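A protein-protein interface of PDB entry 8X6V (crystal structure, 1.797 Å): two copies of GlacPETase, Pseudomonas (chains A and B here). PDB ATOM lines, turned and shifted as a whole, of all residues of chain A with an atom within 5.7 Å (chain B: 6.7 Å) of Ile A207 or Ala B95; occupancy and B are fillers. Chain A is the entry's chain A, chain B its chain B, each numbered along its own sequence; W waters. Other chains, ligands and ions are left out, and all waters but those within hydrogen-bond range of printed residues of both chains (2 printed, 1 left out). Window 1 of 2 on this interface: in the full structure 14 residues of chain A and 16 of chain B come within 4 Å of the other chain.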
ATOM      1  N   ASN A  52      -3.671  31.817 -12.421  1.00  0.00           N
ATOM      2  CA  ASN A  52      -4.632  31.209 -13.327  1.00  0.00           C
ATOM      3  C   ASN A  52      -4.742  32.002 -14.628  1.00  0.00           C
ATOM      4  O   ASN A  52      -4.575  33.226 -14.655  1.00  0.00           O
ATOM      5  CB  ASN A  52      -6.019  31.116 -12.685  1.00  0.00           C
ATOM      6  CG  ASN A  52      -6.084  30.110 -11.546  1.00  0.00           C
ATOM      7  OD1 ASN A  52      -6.740  30.360 -10.541  1.00  0.00           O
ATOM      8  ND2 ASN A  52      -5.421  28.967 -11.707  1.00  0.00           N
ATOM      9  N   GLN A  56      -8.243  28.089 -17.977  1.00  0.00           N
ATOM     10  CA  GLN A  56      -8.539  27.163 -16.894  1.00  0.00           C
ATOM     11  C   GLN A  56      -9.946  27.299 -16.347  1.00  0.00           C
ATOM     12  O   GLN A  56     -10.315  26.529 -15.454  1.00  0.00           O
ATOM     13  CB  GLN A  56      -7.541  27.362 -15.759  1.00  0.00           C
ATOM     14  CG  GLN A  56      -6.131  27.023 -16.157  1.00  0.00           C
ATOM     15  CD  GLN A  56      -5.196  27.194 -15.010  1.00  0.00           C
ATOM     16  OE1 GLN A  56      -4.854  28.313 -14.658  1.00  0.00           O
ATOM     17  NE2 GLN A  56      -4.802  26.081 -14.381  1.00  0.00           N
ATOM     18  N   MET A  57     -10.753  28.227 -16.871  1.00  0.00           N
ATOM     19  CA  MET A  57     -12.082  28.469 -16.331  1.00  0.00           C
ATOM     20  C   MET A  57     -13.192  28.014 -17.275  1.00  0.00           C
ATOM     21  O   MET A  57     -14.366  28.308 -17.021  1.00  0.00           O
ATOM     22  CB  MET A  57     -12.249  29.950 -15.983  1.00  0.00           C
ATOM     23  CG  MET A  57     -11.317  30.451 -14.872  1.00  0.00           C
ATOM     24  SD  MET A  57     -11.454  29.461 -13.361  1.00  0.00           S
ATOM     25  CE  MET A  57     -12.978  30.066 -12.645  1.00  0.00           C
ATOM     26  N   TRP A  59     -14.609  25.196 -17.831  1.00  0.00           N
ATOM     27  CA  TRP A  59     -15.636  24.335 -17.244  1.00  0.00           C
ATOM     28  C   TRP A  59     -16.866  25.145 -16.867  1.00  0.00           C
ATOM     29  O   TRP A  59     -18.004  24.692 -17.050  1.00  0.00           O
ATOM     30  CB  TRP A  59     -15.087  23.602 -16.010  1.00  0.00           C
ATOM     31  CG  TRP A  59     -14.855  24.513 -14.827  1.00  0.00           C
ATOM     32  CD1 TRP A  59     -13.773  25.329 -14.614  1.00  0.00           C
ATOM     33  CD2 TRP A  59     -15.739  24.724 -13.716  1.00  0.00           C
ATOM     34  NE1 TRP A  59     -13.932  26.025 -13.437  1.00  0.00           N
ATOM     35  CE2 TRP A  59     -15.127  25.669 -12.865  1.00  0.00           C
ATOM     36  CE3 TRP A  59     -16.988  24.198 -13.354  1.00  0.00           C
ATOM     37  CZ2 TRP A  59     -15.723  26.104 -11.680  1.00  0.00           C
ATOM     38  CZ3 TRP A  59     -17.575  24.625 -12.177  1.00  0.00           C
ATOM     39  CH2 TRP A  59     -16.944  25.569 -11.353  1.00  0.00           C
ATOM     40  N   PHE A 122     -12.891  33.417  -9.089  1.00  0.00           N
ATOM     41  CA  PHE A 122     -12.374  32.367  -8.211  1.00  0.00           C
ATOM     42  C   PHE A 122     -11.154  32.860  -7.440  1.00  0.00           C
ATOM     43  O   PHE A 122     -10.241  33.440  -8.032  1.00  0.00           O
ATOM     44  CB  PHE A 122     -11.994  31.135  -9.040  1.00  0.00           C
ATOM     45  CG  PHE A 122     -11.099  30.164  -8.325  1.00  0.00           C
ATOM     46  CD1 PHE A 122     -11.514  29.552  -7.156  1.00  0.00           C
ATOM     47  CD2 PHE A 122      -9.840  29.862  -8.834  1.00  0.00           C
ATOM     48  CE1 PHE A 122     -10.681  28.642  -6.491  1.00  0.00           C
ATOM     49  CE2 PHE A 122      -9.005  28.951  -8.188  1.00  0.00           C
ATOM     50  CZ  PHE A 122      -9.431  28.338  -7.006  1.00  0.00           C
ATOM     51  N   HIS A 203      -9.907  23.704  -2.681  1.00  0.00           N
ATOM     52  CA  HIS A 203      -9.726  24.992  -3.348  1.00  0.00           C
ATOM     53  C   HIS A 203      -9.697  24.846  -4.861  1.00  0.00           C
ATOM     54  O   HIS A 203     -10.316  25.639  -5.579  1.00  0.00           O
ATOM     55  CB  HIS A 203      -8.438  25.658  -2.871  1.00  0.00           C
ATOM     56  CG  HIS A 203      -8.338  27.100  -3.268  1.00  0.00           C
ATOM     57  ND1 HIS A 203      -9.259  28.041  -2.862  1.00  0.00           N
ATOM     58  CD2 HIS A 203      -7.435  27.761  -4.031  1.00  0.00           C
ATOM     59  CE1 HIS A 203      -8.916  29.226  -3.340  1.00  0.00           C
ATOM     60  NE2 HIS A 203      -7.821  29.080  -4.064  1.00  0.00           N
ATOM     61  N   LEU A 204      -9.011  23.827  -5.367  1.00  0.00           N
ATOM     62  CA  LEU A 204      -8.865  23.707  -6.812  1.00  0.00           C
ATOM     63  C   LEU A 204     -10.061  23.008  -7.480  1.00  0.00           C
ATOM     64  O   LEU A 204      -9.953  22.583  -8.636  1.00  0.00           O
ATOM     65  CB  LEU A 204      -7.544  23.000  -7.139  1.00  0.00           C
ATOM     66  CG  LEU A 204      -6.351  23.836  -6.638  1.00  0.00           C
ATOM     67  CD1 LEU A 204      -5.016  23.172  -6.945  1.00  0.00           C
ATOM     68  CD2 LEU A 204      -6.403  25.209  -7.236  1.00  0.00           C
ATOM     69  N   ASP A 205     -11.202  22.895  -6.795  1.00  0.00           N
ATOM     70  CA  ASP A 205     -12.399  22.407  -7.473  1.00  0.00           C
ATOM     71  C   ASP A 205     -12.982  23.438  -8.433  1.00  0.00           C
ATOM     72  O   ASP A 205     -13.804  23.079  -9.286  1.00  0.00           O
ATOM     73  CB  ASP A 205     -13.455  21.996  -6.453  1.00  0.00           C
ATOM     74  CG  ASP A 205     -13.203  20.608  -5.879  1.00  0.00           C
ATOM     75  OD1 ASP A 205     -12.494  19.792  -6.514  1.00  0.00           O
ATOM     76  OD2 ASP A 205     -13.723  20.338  -4.787  1.00  0.00           O
ATOM     77  N   TRP A 206     -12.545  24.696  -8.347  1.00  0.00           N
ATOM     78  CA  TRP A 206     -13.098  25.775  -9.155  1.00  0.00           C
ATOM     79  C   TRP A 206     -12.264  26.090 -10.396  1.00  0.00           C
ATOM     80  O   TRP A 206     -12.503  27.117 -11.044  1.00  0.00           O
ATOM     81  CB  TRP A 206     -13.272  27.040  -8.309  1.00  0.00           C
ATOM     82  CG  TRP A 206     -14.509  27.030  -7.434  1.00  0.00           C
ATOM     83  CD1 TRP A 206     -15.757  27.508  -7.757  1.00  0.00           C
ATOM     84  CD2 TRP A 206     -14.607  26.526  -6.098  1.00  0.00           C
ATOM     85  NE1 TRP A 206     -16.628  27.306  -6.701  1.00  0.00           N
ATOM     86  CE2 TRP A 206     -15.940  26.717  -5.670  1.00  0.00           C
ATOM     87  CE3 TRP A 206     -13.693  25.930  -5.216  1.00  0.00           C
ATOM     88  CZ2 TRP A 206     -16.379  26.338  -4.400  1.00  0.00           C
ATOM     89  CZ3 TRP A 206     -14.141  25.530  -3.960  1.00  0.00           C
ATOM     90  CH2 TRP A 206     -15.470  25.735  -3.567  1.00  0.00           C
ATOM     91  N   ILE A 207     -11.317  25.225 -10.758  1.00  0.00           N
ATOM     92  CA  ILE A 207     -10.643  25.279 -12.050  1.00  0.00           C
ATOM     93  C   ILE A 207     -10.891  23.951 -12.770  1.00  0.00           C
ATOM     94  O   ILE A 207     -11.468  23.023 -12.209  1.00  0.00           O
ATOM     95  CB  ILE A 207      -9.137  25.585 -11.913  1.00  0.00           C
ATOM     96  CG1 ILE A 207      -8.457  24.536 -11.032  1.00  0.00           C
ATOM     97  CG2 ILE A 207      -8.950  26.979 -11.345  1.00  0.00           C
ATOM     98  CD1 ILE A 207      -6.946  24.700 -10.977  1.00  0.00           C
ATOM     99  N   ASN A 208     -10.477  23.878 -14.043  1.00  0.00           N
ATOM    100  CA  ASN A 208     -10.903  22.759 -14.892  1.00  0.00           C
ATOM    101  C   ASN A 208     -10.536  21.399 -14.303  1.00  0.00           C
ATOM    102  O   ASN A 208     -11.270  20.421 -14.497  1.00  0.00           O
ATOM    103  CB  ASN A 208     -10.286  22.873 -16.283  1.00  0.00           C
ATOM    104  CG  ASN A 208     -11.001  23.858 -17.150  1.00  0.00           C
ATOM    105  OD1 ASN A 208     -12.166  24.163 -16.918  1.00  0.00           O
ATOM    106  ND2 ASN A 208     -10.307  24.368 -18.167  1.00  0.00           N
ATOM    107  N   THR A 209      -9.413  21.308 -13.607  1.00  0.00           N
ATOM    108  CA  THR A 209      -8.983  20.034 -13.048  1.00  0.00           C
ATOM    109  C   THR A 209      -9.670  19.691 -11.732  1.00  0.00           C
ATOM    110  O   THR A 209      -9.289  18.701 -11.095  1.00  0.00           O
ATOM    111  CB  THR A 209      -7.463  20.025 -12.858  1.00  0.00           C
ATOM    112  OG1 THR A 209      -7.084  21.061 -11.951  1.00  0.00           O
ATOM    113  CG2 THR A 209      -6.786  20.288 -14.168  1.00  0.00           C
ATOM    114  N   GLY A 210     -10.666  20.461 -11.314  1.00  0.00           N
ATOM    115  CA  GLY A 210     -11.433  20.109 -10.131  1.00  0.00           C
ATOM    116  C   GLY A 210     -12.204  18.810 -10.318  1.00  0.00           C
ATOM    117  O   GLY A 210     -12.332  18.269 -11.413  1.00  0.00           O
ATOM    118  N   GLN A 215     -18.032  19.563  -9.085  1.00  0.00           N
ATOM    119  CA  GLN A 215     -18.257  20.711  -9.959  1.00  0.00           C
ATOM    120  C   GLN A 215     -19.706  20.776 -10.427  1.00  0.00           C
ATOM    121  O   GLN A 215     -20.246  21.867 -10.622  1.00  0.00           O
ATOM    122  CB  GLN A 215     -17.313  20.661 -11.154  1.00  0.00           C
ATOM    123  CG  GLN A 215     -15.861  21.065 -10.809  1.00  0.00           C
ATOM    124  CD  GLN A 215     -15.032  21.304 -12.045  1.00  0.00           C
ATOM    125  OE1 GLN A 215     -15.342  20.784 -13.123  1.00  0.00           O
ATOM    126  NE2 GLN A 215     -13.973  22.104 -11.909  1.00  0.00           N
ATOM    127  N   HIS B  90      -0.112  18.229  -5.462  1.00  0.00           N
ATOM    128  CA  HIS B  90      -0.215  17.474  -6.707  1.00  0.00           C
ATOM    129  C   HIS B  90      -1.246  18.093  -7.652  1.00  0.00           C
ATOM    130  O   HIS B  90      -0.994  18.245  -8.851  1.00  0.00           O
ATOM    131  CB  HIS B  90      -0.582  16.018  -6.393  1.00  0.00           C
ATOM    132  CG  HIS B  90       0.568  15.194  -5.900  1.00  0.00           C
ATOM    133  ND1 HIS B  90       1.691  14.952  -6.662  1.00  0.00           N
ATOM    134  CD2 HIS B  90       0.759  14.536  -4.731  1.00  0.00           C
ATOM    135  CE1 HIS B  90       2.527  14.188  -5.982  1.00  0.00           C
ATOM    136  NE2 HIS B  90       1.985  13.919  -4.808  1.00  0.00           N
ATOM    137  N   LYS B  91      -2.425  18.430  -7.132  1.00  0.00           N
ATOM    138  CA  LYS B  91      -3.441  19.058  -7.968  1.00  0.00           C
ATOM    139  C   LYS B  91      -2.953  20.405  -8.479  1.00  0.00           C
ATOM    140  O   LYS B  91      -3.252  20.799  -9.614  1.00  0.00           O
ATOM    141  CB  LYS B  91      -4.735  19.223  -7.172  1.00  0.00           C
ATOM    142  CG  LYS B  91      -5.448  17.923  -6.825  1.00  0.00           C
ATOM    143  CD  LYS B  91      -6.506  18.214  -5.786  1.00  0.00           C
ATOM    144  CE  LYS B  91      -7.539  17.105  -5.677  1.00  0.00           C
ATOM    145  NZ  LYS B  91      -8.521  17.469  -4.613  1.00  0.00           N
ATOM    146  N   ALA B  92      -2.194  21.122  -7.645  1.00  0.00           N
ATOM    147  CA  ALA B  92      -1.632  22.402  -8.062  1.00  0.00           C
ATOM    148  C   ALA B  92      -0.556  22.220  -9.123  1.00  0.00           C
ATOM    149  O   ALA B  92      -0.398  23.085  -9.997  1.00  0.00           O
ATOM    150  CB  ALA B  92      -1.082  23.147  -6.855  1.00  0.00           C
ATOM    151  N   GLY B  93       0.184  21.108  -9.069  1.00  0.00           N
ATOM    152  CA  GLY B  93       1.132  20.814 -10.130  1.00  0.00           C
ATOM    153  C   GLY B  93       0.452  20.566 -11.460  1.00  0.00           C
ATOM    154  O   GLY B  93       0.872  21.086 -12.499  1.00  0.00           O
ATOM    155  N   ILE B  94      -0.615  19.763 -11.449  1.00  0.00           N
ATOM    156  CA  ILE B  94      -1.395  19.560 -12.663  1.00  0.00           C
ATOM    157  C   ILE B  94      -1.960  20.888 -13.161  1.00  0.00           C
ATOM    158  O   ILE B  94      -1.914  21.190 -14.359  1.00  0.00           O
ATOM    159  CB  ILE B  94      -2.507  18.526 -12.405  1.00  0.00           C
ATOM    160  CG1 ILE B  94      -1.895  17.166 -12.047  1.00  0.00           C
ATOM    161  CG2 ILE B  94      -3.452  18.448 -13.607  1.00  0.00           C
ATOM    162  CD1 ILE B  94      -1.130  16.484 -13.183  1.00  0.00           C
ATOM    163  N   ALA B  95      -2.488  21.708 -12.249  1.00  0.00           N
ATOM    164  CA  ALA B  95      -3.031  23.003 -12.654  1.00  0.00           C
ATOM    165  C   ALA B  95      -1.950  23.877 -13.276  1.00  0.00           C
ATOM    166  O   ALA B  95      -2.166  24.501 -14.322  1.00  0.00           O
ATOM    167  CB  ALA B  95      -3.656  23.713 -11.457  1.00  0.00           C
ATOM    168  N   LYS B  96      -0.769  23.903 -12.657  1.00  0.00           N
ATOM    169  CA  LYS B  96       0.320  24.738 -13.154  1.00  0.00           C
ATOM    170  C   LYS B  96       0.776  24.301 -14.539  1.00  0.00           C
ATOM    171  O   LYS B  96       1.026  25.142 -15.409  1.00  0.00           O
ATOM    172  CB  LYS B  96       1.483  24.710 -12.164  1.00  0.00           C
ATOM    173  CG  LYS B  96       2.725  25.465 -12.628  1.00  0.00           C
ATOM    174  CD  LYS B  96       2.400  26.908 -12.993  1.00  0.00           C
ATOM    175  CE  LYS B  96       2.235  27.795 -11.756  1.00  0.00           C
ATOM    176  NZ  LYS B  96       2.262  29.269 -12.117  1.00  0.00           N
ATOM    177  N   LEU B  97       0.889  22.988 -14.765  1.00  0.00           N
ATOM    178  CA  LEU B  97       1.263  22.491 -16.085  1.00  0.00           C
ATOM    179  C   LEU B  97       0.254  22.933 -17.140  1.00  0.00           C
ATOM    180  O   LEU B  97       0.629  23.354 -18.239  1.00  0.00           O
ATOM    181  CB  LEU B  97       1.365  20.965 -16.064  1.00  0.00           C
ATOM    182  CG  LEU B  97       2.537  20.354 -15.287  1.00  0.00           C
ATOM    183  CD1 LEU B  97       2.415  18.840 -15.263  1.00  0.00           C
ATOM    184  CD2 LEU B  97       3.870  20.777 -15.895  1.00  0.00           C
ATOM    185  N   ARG B  98      -1.037  22.819 -16.832  1.00  0.00           N
ATOM    186  CA  ARG B  98      -2.041  23.264 -17.794  1.00  0.00           C
ATOM    187  C   ARG B  98      -1.971  24.768 -18.004  1.00  0.00           C
ATOM    188  O   ARG B  98      -2.103  25.247 -19.135  1.00  0.00           O
ATOM    189  CB  ARG B  98      -3.428  22.845 -17.330  1.00  0.00           C
ATOM    190  CG  ARG B  98      -3.705  21.397 -17.642  1.00  0.00           C
ATOM    191  CD  ARG B  98      -4.845  20.911 -16.847  1.00  0.00           C
ATOM    192  NE  ARG B  98      -5.316  19.625 -17.323  1.00  0.00           N
ATOM    193  CZ  ARG B  98      -6.439  19.468 -18.005  1.00  0.00           C
ATOM    194  NH1 ARG B  98      -7.188  20.526 -18.284  1.00  0.00           N
ATOM    195  NH2 ARG B  98      -6.813  18.260 -18.402  1.00  0.00           N
ATOM    196  N   SER B  99      -1.754  25.517 -16.920  1.00  0.00           N
ATOM    197  CA  SER B  99      -1.572  26.962 -17.010  1.00  0.00           C
ATOM    198  C   SER B  99      -0.355  27.309 -17.858  1.00  0.00           C
ATOM    199  O   SER B  99      -0.428  28.168 -18.747  1.00  0.00           O
ATOM    200  CB  SER B  99      -1.438  27.548 -15.603  1.00  0.00           C
ATOM    201  OG  SER B  99      -1.273  28.957 -15.628  1.00  0.00           O
ATOM    202  N   GLU B 100       0.778  26.639 -17.599  1.00  0.00           N
ATOM    203  CA  GLU B 100       1.990  26.897 -18.372  1.00  0.00           C
ATOM    204  C   GLU B 100       1.806  26.574 -19.850  1.00  0.00           C
ATOM    205  O   GLU B 100       2.440  27.206 -20.701  1.00  0.00           O
ATOM    206  CB  GLU B 100       3.165  26.098 -17.806  1.00  0.00           C
ATOM    207  CG  GLU B 100       3.658  26.594 -16.465  1.00  0.00           C
ATOM    208  CD  GLU B 100       4.324  27.946 -16.566  1.00  0.00           C
ATOM    209  OE1 GLU B 100       5.515  27.996 -16.933  1.00  0.00           O
ATOM    210  OE2 GLU B 100       3.647  28.957 -16.289  1.00  0.00           O
ATOM    211  N   PHE B 117      -0.481  12.943 -18.317  1.00  0.00           N
ATOM    212  CA  PHE B 117      -0.004  13.506 -17.061  1.00  0.00           C
ATOM    213  C   PHE B 117       0.021  12.427 -15.981  1.00  0.00           C
ATOM    214  O   PHE B 117      -0.876  11.577 -15.911  1.00  0.00           O
ATOM    215  CB  PHE B 117      -0.893  14.661 -16.590  1.00  0.00           C
ATOM    216  CG  PHE B 117      -0.670  15.962 -17.322  1.00  0.00           C
ATOM    217  CD1 PHE B 117       0.306  16.080 -18.305  1.00  0.00           C
ATOM    218  CD2 PHE B 117      -1.429  17.077 -17.002  1.00  0.00           C
ATOM    219  CE1 PHE B 117       0.509  17.288 -18.971  1.00  0.00           C
ATOM    220  CE2 PHE B 117      -1.225  18.295 -17.662  1.00  0.00           C
ATOM    221  CZ  PHE B 117      -0.255  18.395 -18.642  1.00  0.00           C
HETATM  222  O   HOH W   1      -7.065  23.686 -17.841  1.00  0.00           O
HETATM  223  O   HOH W   2     -10.000  19.009  -6.409  1.00  0.00           O
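No position is printed for both chains. Of the 7 pairs that touch across the chains among the printed residues, none has its exchanged pair printed and touching as well.
The side-chain amide nitrogen (NE2) of Gln A56 sits at hydrogen-bond distance from the backbone carbonyl oxygen (O) of Ala B95 (3.1 Å).
Among the printed residues, pairs that only touch across the chains: Gln A56 with Ser B99 (3.6 Å), Leu A204 with Lys B91 (3.8 Å), Leu A204 with Ala B92 (3.6 Å), Ile A207 with Ala B95 (3.5 Å), Thr A209 with Ile B94 (3.8 Å) and Thr A209 with Arg B98 (3.4 Å).
Hydrophobic or aromatic side chains of chain B that line the printed part of chain A: Ala B92, Ile B94 and Ala B95. Of the 14 printed residues of chain A, 4 touch a printed residue of chain B. Printed residues of chain A that touch a printed residue of chain B: Gln A56, Leu A204, Ile A207 and Thr A209. Hydrophobic or aromatic side chains of chain A within 4 Å of the printed part of chain B: Leu A204 and Ile A207.
Of the printed residues of chain B, Gln A56 touches Ala B95 (3.1 Å) and Ser B99 (3.6 Å). Of the printed residues of chain B, Leu A204 touches Lys B91 and Ala B92. Ile A207 touches just one residue of chain B: Ala B95 (3.5 Å). Of the printed residues of chain A, Ala B92 touches Leu A204. Of chain A, only Gln A56 and Ile A207 come within 4 Å of Ala B95. Printed residues of chain A within 4 Å of Arg B98: Thr A209 (3.4 Å). The nearest residue of chain A that does not touch Ala B95 is Thr A209 (4.4 Å).
Water W2 lies within hydrogen-bond range of the side-chain carboxylate (OD1) of Asp A205 (2.6 Å) and the side-chain amino group (NZ) of Lys B91 (2.8 Å). Water W1 bridges the guanidinium group of Arg B98 and the side-chain amide nitrogen of Asn A208.
ND2 of Asn A52 is in hydrogen-bond range of OE1 of Gln A56. The backbone carbonyl oxygen of Gln A56 lies within hydrogen-bond range of the backbone NH of Asn A208 (3.0 Å). O of Leu A204 sits close to N of Gly A210. O of Ile A207 sits at hydrogen-bond distance from NE2 of Gln A215, 2.7 Å away.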
